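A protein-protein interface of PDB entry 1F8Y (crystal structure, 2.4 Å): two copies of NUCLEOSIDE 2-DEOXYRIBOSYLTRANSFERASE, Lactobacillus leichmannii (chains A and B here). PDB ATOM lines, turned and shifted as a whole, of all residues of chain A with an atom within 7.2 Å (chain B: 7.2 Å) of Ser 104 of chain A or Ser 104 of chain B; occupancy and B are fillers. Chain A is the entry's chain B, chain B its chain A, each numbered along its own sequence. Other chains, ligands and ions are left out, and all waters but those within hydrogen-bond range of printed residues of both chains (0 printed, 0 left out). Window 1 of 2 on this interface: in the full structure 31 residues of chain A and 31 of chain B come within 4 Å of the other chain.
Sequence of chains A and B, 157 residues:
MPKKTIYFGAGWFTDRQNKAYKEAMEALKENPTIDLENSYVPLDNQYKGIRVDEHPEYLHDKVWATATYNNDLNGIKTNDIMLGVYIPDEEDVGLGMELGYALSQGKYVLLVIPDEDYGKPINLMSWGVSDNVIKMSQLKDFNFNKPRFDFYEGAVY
Of the 12 printed residues of chain A, 1 touches a printed residue of chain B.
Printed residues of chain B that touch a printed residue of chain A: Ser 104.
Among the printed residues, no Asp or Glu carboxylate lies within 4 Å of a Lys or Arg side-chain nitrogen of the other chain.
OG of Ser 104 of chain B is in hydrogen-bond range of O of Tyr 101 of chain B (2.6 Å).
NE2 of Gln 105 of chain B is in hydrogen-bond range of OG of Ser 104 of chain B (3.1 Å).
The side-chain hydroxyl (OG) of Ser 104 of chain A sits at hydrogen-bond distance from the backbone carbonyl oxygen (O) of Tyr 101 of chain A, at 2.6 Å.
Ser 104 of chain B touches just one residue of chain A: Ser 104 (3.3 Å).
The nearest residue of chain A that does not touch Ser 104 of chain B is Gly 100 of chain A (5.2 Å).
Ser 104 of chain B touches its own counterpart, Ser 104 of chain A.
10 positions are printed for both chains.
Among the printed residues, merely in contact across the chains: Ser 104 of chain A with Ser 104 of chain B.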
ATOM      1  N   ILE A  76     -20.364 -28.668  32.588  1.00  0.00           N
ATOM      2  CA  ILE A  76     -21.550 -28.802  31.757  1.00  0.00           C
ATOM      3  C   ILE A  76     -21.717 -30.180  31.146  1.00  0.00           C
ATOM      4  O   ILE A  76     -22.741 -30.828  31.359  1.00  0.00           O
ATOM      5  CB  ILE A  76     -21.597 -27.731  30.638  1.00  0.00           C
ATOM      6  CG1 ILE A  76     -21.820 -26.345  31.252  1.00  0.00           C
ATOM      7  CG2 ILE A  76     -22.708 -28.044  29.643  1.00  0.00           C
ATOM      8  CD1 ILE A  76     -21.659 -25.208  30.272  1.00  0.00           C
ATOM      9  N   GLU A  98     -22.958 -20.622  27.412  1.00  0.00           N
ATOM     10  CA  GLU A  98     -23.163 -21.924  28.044  1.00  0.00           C
ATOM     11  C   GLU A  98     -24.431 -22.627  27.572  1.00  0.00           C
ATOM     12  O   GLU A  98     -24.466 -23.857  27.489  1.00  0.00           O
ATOM     13  CB  GLU A  98     -23.132 -21.779  29.564  1.00  0.00           C
ATOM     14  CG  GLU A  98     -21.770 -21.293  30.064  1.00  0.00           C
ATOM     15  CD  GLU A  98     -21.781 -20.808  31.501  1.00  0.00           C
ATOM     16  OE1 GLU A  98     -20.682 -20.686  32.089  1.00  0.00           O
ATOM     17  OE2 GLU A  98     -22.870 -20.535  32.042  1.00  0.00           O
ATOM     18  N   LEU A  99     -25.457 -21.856  27.221  1.00  0.00           N
ATOM     19  CA  LEU A  99     -26.695 -22.448  26.727  1.00  0.00           C
ATOM     20  C   LEU A  99     -26.364 -23.128  25.392  1.00  0.00           C
ATOM     21  O   LEU A  99     -26.747 -24.285  25.157  1.00  0.00           O
ATOM     22  CB  LEU A  99     -27.769 -21.370  26.531  1.00  0.00           C
ATOM     23  CG  LEU A  99     -28.287 -20.635  27.779  1.00  0.00           C
ATOM     24  CD1 LEU A  99     -29.183 -19.489  27.375  1.00  0.00           C
ATOM     25  CD2 LEU A  99     -29.037 -21.572  28.703  1.00  0.00           C
ATOM     26  N   GLY A 100     -25.602 -22.419  24.552  1.00  0.00           N
ATOM     27  CA  GLY A 100     -25.199 -22.945  23.255  1.00  0.00           C
ATOM     28  C   GLY A 100     -24.317 -24.178  23.408  1.00  0.00           C
ATOM     29  O   GLY A 100     -24.490 -25.172  22.696  1.00  0.00           O
ATOM     30  N   TYR A 101     -23.378 -24.121  24.346  1.00  0.00           N
ATOM     31  CA  TYR A 101     -22.495 -25.252  24.610  1.00  0.00           C
ATOM     32  C   TYR A 101     -23.324 -26.448  25.127  1.00  0.00           C
ATOM     33  O   TYR A 101     -23.088 -27.594  24.740  1.00  0.00           O
ATOM     34  CB  TYR A 101     -21.426 -24.873  25.640  1.00  0.00           C
ATOM     35  CG  TYR A 101     -20.432 -25.979  25.857  1.00  0.00           C
ATOM     36  CD1 TYR A 101     -20.481 -26.778  26.999  1.00  0.00           C
ATOM     37  CD2 TYR A 101     -19.501 -26.296  24.873  1.00  0.00           C
ATOM     38  CE1 TYR A 101     -19.630 -27.875  27.148  1.00  0.00           C
ATOM     39  CE2 TYR A 101     -18.648 -27.388  25.014  1.00  0.00           C
ATOM     40  CZ  TYR A 101     -18.719 -28.171  26.148  1.00  0.00           C
ATOM     41  OH  TYR A 101     -17.890 -29.262  26.258  1.00  0.00           O
ATOM     42  N   ALA A 102     -24.320 -26.170  25.967  1.00  0.00           N
ATOM     43  CA  ALA A 102     -25.166 -27.229  26.507  1.00  0.00           C
ATOM     44  C   ALA A 102     -25.894 -27.921  25.357  1.00  0.00           C
ATOM     45  O   ALA A 102     -26.004 -29.146  25.340  1.00  0.00           O
ATOM     46  CB  ALA A 102     -26.164 -26.663  27.505  1.00  0.00           C
ATOM     47  N   LEU A 103     -26.378 -27.127  24.400  1.00  0.00           N
ATOM     48  CA  LEU A 103     -27.086 -27.646  23.224  1.00  0.00           C
ATOM     49  C   LEU A 103     -26.172 -28.630  22.502  1.00  0.00           C
ATOM     50  O   LEU A 103     -26.572 -29.754  22.209  1.00  0.00           O
ATOM     51  CB  LEU A 103     -27.425 -26.500  22.268  1.00  0.00           C
ATOM     52  CG  LEU A 103     -28.564 -26.518  21.235  1.00  0.00           C
ATOM     53  CD1 LEU A 103     -28.117 -25.712  20.043  1.00  0.00           C
ATOM     54  CD2 LEU A 103     -28.962 -27.899  20.782  1.00  0.00           C
ATOM     55  N   SER A 104     -24.938 -28.211  22.240  1.00  0.00           N
ATOM     56  CA  SER A 104     -23.980 -29.057  21.544  1.00  0.00           C
ATOM     57  C   SER A 104     -23.736 -30.349  22.313  1.00  0.00           C
ATOM     58  O   SER A 104     -23.569 -31.412  21.721  1.00  0.00           O
ATOM     59  CB  SER A 104     -22.651 -28.322  21.353  1.00  0.00           C
ATOM     60  OG  SER A 104     -21.907 -28.277  22.562  1.00  0.00           O
ATOM     61  N   GLN A 105     -23.706 -30.252  23.637  1.00  0.00           N
ATOM     62  CA  GLN A 105     -23.488 -31.419  24.479  1.00  0.00           C
ATOM     63  C   GLN A 105     -24.731 -32.287  24.635  1.00  0.00           C
ATOM     64  O   GLN A 105     -24.694 -33.305  25.315  1.00  0.00           O
ATOM     65  CB  GLN A 105     -22.978 -30.984  25.846  1.00  0.00           C
ATOM     66  CG  GLN A 105     -21.615 -30.364  25.767  1.00  0.00           C
ATOM     67  CD  GLN A 105     -20.633 -31.269  25.054  1.00  0.00           C
ATOM     68  OE1 GLN A 105     -19.973 -30.864  24.112  1.00  0.00           O
ATOM     69  NE2 GLN A 105     -20.554 -32.511  25.493  1.00  0.00           N
ATOM     70  N   GLY A 106     -25.833 -31.869  24.023  1.00  0.00           N
ATOM     71  CA  GLY A 106     -27.058 -32.632  24.096  1.00  0.00           C
ATOM     72  C   GLY A 106     -27.731 -32.668  25.448  1.00  0.00           C
ATOM     73  O   GLY A 106     -28.415 -33.638  25.760  1.00  0.00           O
ATOM     74  N   LYS A 107     -27.562 -31.614  26.241  1.00  0.00           N
ATOM     75  CA  LYS A 107     -28.165 -31.540  27.568  1.00  0.00           C
ATOM     76  C   LYS A 107     -29.537 -30.873  27.532  1.00  0.00           C
ATOM     77  O   LYS A 107     -29.851 -30.112  26.612  1.00  0.00           O
ATOM     78  CB  LYS A 107     -27.281 -30.722  28.506  1.00  0.00           C
ATOM     79  CG  LYS A 107     -25.848 -31.193  28.606  1.00  0.00           C
ATOM     80  CD  LYS A 107     -25.770 -32.572  29.211  1.00  0.00           C
ATOM     81  CE  LYS A 107     -24.348 -33.061  29.242  1.00  0.00           C
ATOM     82  NZ  LYS A 107     -24.297 -34.419  29.832  1.00  0.00           N
ATOM     83  N   VAL A 129     -33.078 -21.812  22.285  1.00  0.00           N
ATOM     84  CA  VAL A 129     -32.169 -22.869  22.709  1.00  0.00           C
ATOM     85  C   VAL A 129     -32.704 -23.652  23.923  1.00  0.00           C
ATOM     86  O   VAL A 129     -32.227 -24.749  24.229  1.00  0.00           O
ATOM     87  CB  VAL A 129     -30.777 -22.290  23.021  1.00  0.00           C
ATOM     88  CG1 VAL A 129     -30.814 -21.500  24.331  1.00  0.00           C
ATOM     89  CG2 VAL A 129     -29.736 -23.388  23.062  1.00  0.00           C
ATOM     90  N   GLU B  98     -24.944 -17.685  20.232  1.00  0.00           N
ATOM     91  CA  GLU B  98     -24.457 -17.912  18.883  1.00  0.00           C
ATOM     92  C   GLU B  98     -22.991 -18.284  18.826  1.00  0.00           C
ATOM     93  O   GLU B  98     -22.586 -19.024  17.926  1.00  0.00           O
ATOM     94  CB  GLU B  98     -24.764 -16.707  18.002  1.00  0.00           C
ATOM     95  CG  GLU B  98     -26.244 -16.609  17.662  1.00  0.00           C
ATOM     96  CD  GLU B  98     -26.647 -15.250  17.132  1.00  0.00           C
ATOM     97  OE1 GLU B  98     -27.808 -15.126  16.676  1.00  0.00           O
ATOM     98  OE2 GLU B  98     -25.817 -14.309  17.175  1.00  0.00           O
ATOM     99  N   LEU B  99     -22.191 -17.786  19.770  1.00  0.00           N
ATOM    100  CA  LEU B  99     -20.771 -18.138  19.808  1.00  0.00           C
ATOM    101  C   LEU B  99     -20.679 -19.614  20.153  1.00  0.00           C
ATOM    102  O   LEU B  99     -19.946 -20.382  19.501  1.00  0.00           O
ATOM    103  CB  LEU B  99     -20.016 -17.317  20.851  1.00  0.00           C
ATOM    104  CG  LEU B  99     -20.003 -15.808  20.596  1.00  0.00           C
ATOM    105  CD1 LEU B  99     -19.137 -15.109  21.622  1.00  0.00           C
ATOM    106  CD2 LEU B  99     -19.494 -15.527  19.189  1.00  0.00           C
ATOM    107  N   GLY B 100     -21.463 -20.019  21.151  1.00  0.00           N
ATOM    108  CA  GLY B 100     -21.479 -21.411  21.564  1.00  0.00           C
ATOM    109  C   GLY B 100     -21.910 -22.291  20.406  1.00  0.00           C
ATOM    110  O   GLY B 100     -21.281 -23.316  20.114  1.00  0.00           O
ATOM    111  N   TYR B 101     -22.976 -21.882  19.726  1.00  0.00           N
ATOM    112  CA  TYR B 101     -23.475 -22.642  18.591  1.00  0.00           C
ATOM    113  C   TYR B 101     -22.417 -22.722  17.482  1.00  0.00           C
ATOM    114  O   TYR B 101     -22.204 -23.786  16.918  1.00  0.00           O
ATOM    115  CB  TYR B 101     -24.780 -22.044  18.056  1.00  0.00           C
ATOM    116  CG  TYR B 101     -25.353 -22.823  16.894  1.00  0.00           C
ATOM    117  CD1 TYR B 101     -25.221 -22.367  15.592  1.00  0.00           C
ATOM    118  CD2 TYR B 101     -25.970 -24.048  17.098  1.00  0.00           C
ATOM    119  CE1 TYR B 101     -25.680 -23.118  14.523  1.00  0.00           C
ATOM    120  CE2 TYR B 101     -26.431 -24.804  16.039  1.00  0.00           C
ATOM    121  CZ  TYR B 101     -26.283 -24.336  14.758  1.00  0.00           C
ATOM    122  OH  TYR B 101     -26.739 -25.098  13.709  1.00  0.00           O
ATOM    123  N   ALA B 102     -21.742 -21.611  17.191  1.00  0.00           N
ATOM    124  CA  ALA B 102     -20.691 -21.591  16.164  1.00  0.00           C
ATOM    125  C   ALA B 102     -19.574 -22.579  16.529  1.00  0.00           C
ATOM    126  O   ALA B 102     -19.046 -23.285  15.658  1.00  0.00           O
ATOM    127  CB  ALA B 102     -20.124 -20.196  16.009  1.00  0.00           C
ATOM    128  N   LEU B 103     -19.220 -22.632  17.812  1.00  0.00           N
ATOM    129  CA  LEU B 103     -18.193 -23.557  18.278  1.00  0.00           C
ATOM    130  C   LEU B 103     -18.619 -24.988  17.968  1.00  0.00           C
ATOM    131  O   LEU B 103     -17.804 -25.808  17.547  1.00  0.00           O
ATOM    132  CB  LEU B 103     -17.987 -23.444  19.797  1.00  0.00           C
ATOM    133  CG  LEU B 103     -17.073 -24.497  20.458  1.00  0.00           C
ATOM    134  CD1 LEU B 103     -15.621 -24.227  20.098  1.00  0.00           C
ATOM    135  CD2 LEU B 103     -17.231 -24.474  21.975  1.00  0.00           C
ATOM    136  N   SER B 104     -19.897 -25.286  18.197  1.00  0.00           N
ATOM    137  CA  SER B 104     -20.413 -26.627  17.978  1.00  0.00           C
ATOM    138  C   SER B 104     -20.363 -27.013  16.518  1.00  0.00           C
ATOM    139  O   SER B 104     -20.283 -28.196  16.196  1.00  0.00           O
ATOM    140  CB  SER B 104     -21.844 -26.764  18.505  1.00  0.00           C
ATOM    141  OG  SER B 104     -22.792 -26.190  17.623  1.00  0.00           O
ATOM    142  N   GLN B 105     -20.458 -26.017  15.641  1.00  0.00           N
ATOM    143  CA  GLN B 105     -20.404 -26.268  14.208  1.00  0.00           C
ATOM    144  C   GLN B 105     -18.979 -26.201  13.667  1.00  0.00           C
ATOM    145  O   GLN B 105     -18.766 -26.317  12.470  1.00  0.00           O
ATOM    146  CB  GLN B 105     -21.281 -25.279  13.450  1.00  0.00           C
ATOM    147  CG  GLN B 105     -22.731 -25.284  13.866  1.00  0.00           C
ATOM    148  CD  GLN B 105     -23.364 -26.642  13.748  1.00  0.00           C
ATOM    149  OE1 GLN B 105     -23.392 -27.242  12.678  1.00  0.00           O
ATOM    150  NE2 GLN B 105     -23.862 -27.148  14.857  1.00  0.00           N
ATOM    151  N   GLY B 106     -18.009 -25.968  14.539  1.00  0.00           N
ATOM    152  CA  GLY B 106     -16.623 -25.904  14.103  1.00  0.00           C
ATOM    153  C   GLY B 106     -16.241 -24.728  13.227  1.00  0.00           C
ATOM    154  O   GLY B 106     -15.404 -24.861  12.337  1.00  0.00           O
ATOM    155  N   LYS B 107     -16.837 -23.572  13.473  1.00  0.00           N
ATOM    156  CA  LYS B 107     -16.527 -22.372  12.689  1.00  0.00           C
ATOM    157  C   LYS B 107     -15.437 -21.545  13.389  1.00  0.00           C
ATOM    158  O   LYS B 107     -15.214 -21.688  14.592  1.00  0.00           O
ATOM    159  CB  LYS B 107     -17.782 -21.505  12.549  1.00  0.00           C
ATOM    160  CG  LYS B 107     -19.000 -22.226  11.985  1.00  0.00           C
ATOM    161  CD  LYS B 107     -18.853 -22.493  10.495  1.00  0.00           C
ATOM    162  CE  LYS B 107     -20.013 -23.293   9.990  1.00  0.00           C
ATOM    163  NZ  LYS B 107     -19.837 -23.607   8.566  1.00  0.00           N
ATOM    164  N   VAL B 109     -14.275 -18.429  15.125  1.00  0.00           N
ATOM    165  CA  VAL B 109     -15.014 -17.411  15.860  1.00  0.00           C
ATOM    166  C   VAL B 109     -14.126 -16.195  16.071  1.00  0.00           C
ATOM    167  O   VAL B 109     -13.154 -16.249  16.830  1.00  0.00           O
ATOM    168  CB  VAL B 109     -15.498 -17.941  17.240  1.00  0.00           C
ATOM    169  CG1 VAL B 109     -16.235 -16.850  17.997  1.00  0.00           C
ATOM    170  CG2 VAL B 109     -16.384 -19.169  17.059  1.00  0.00           C
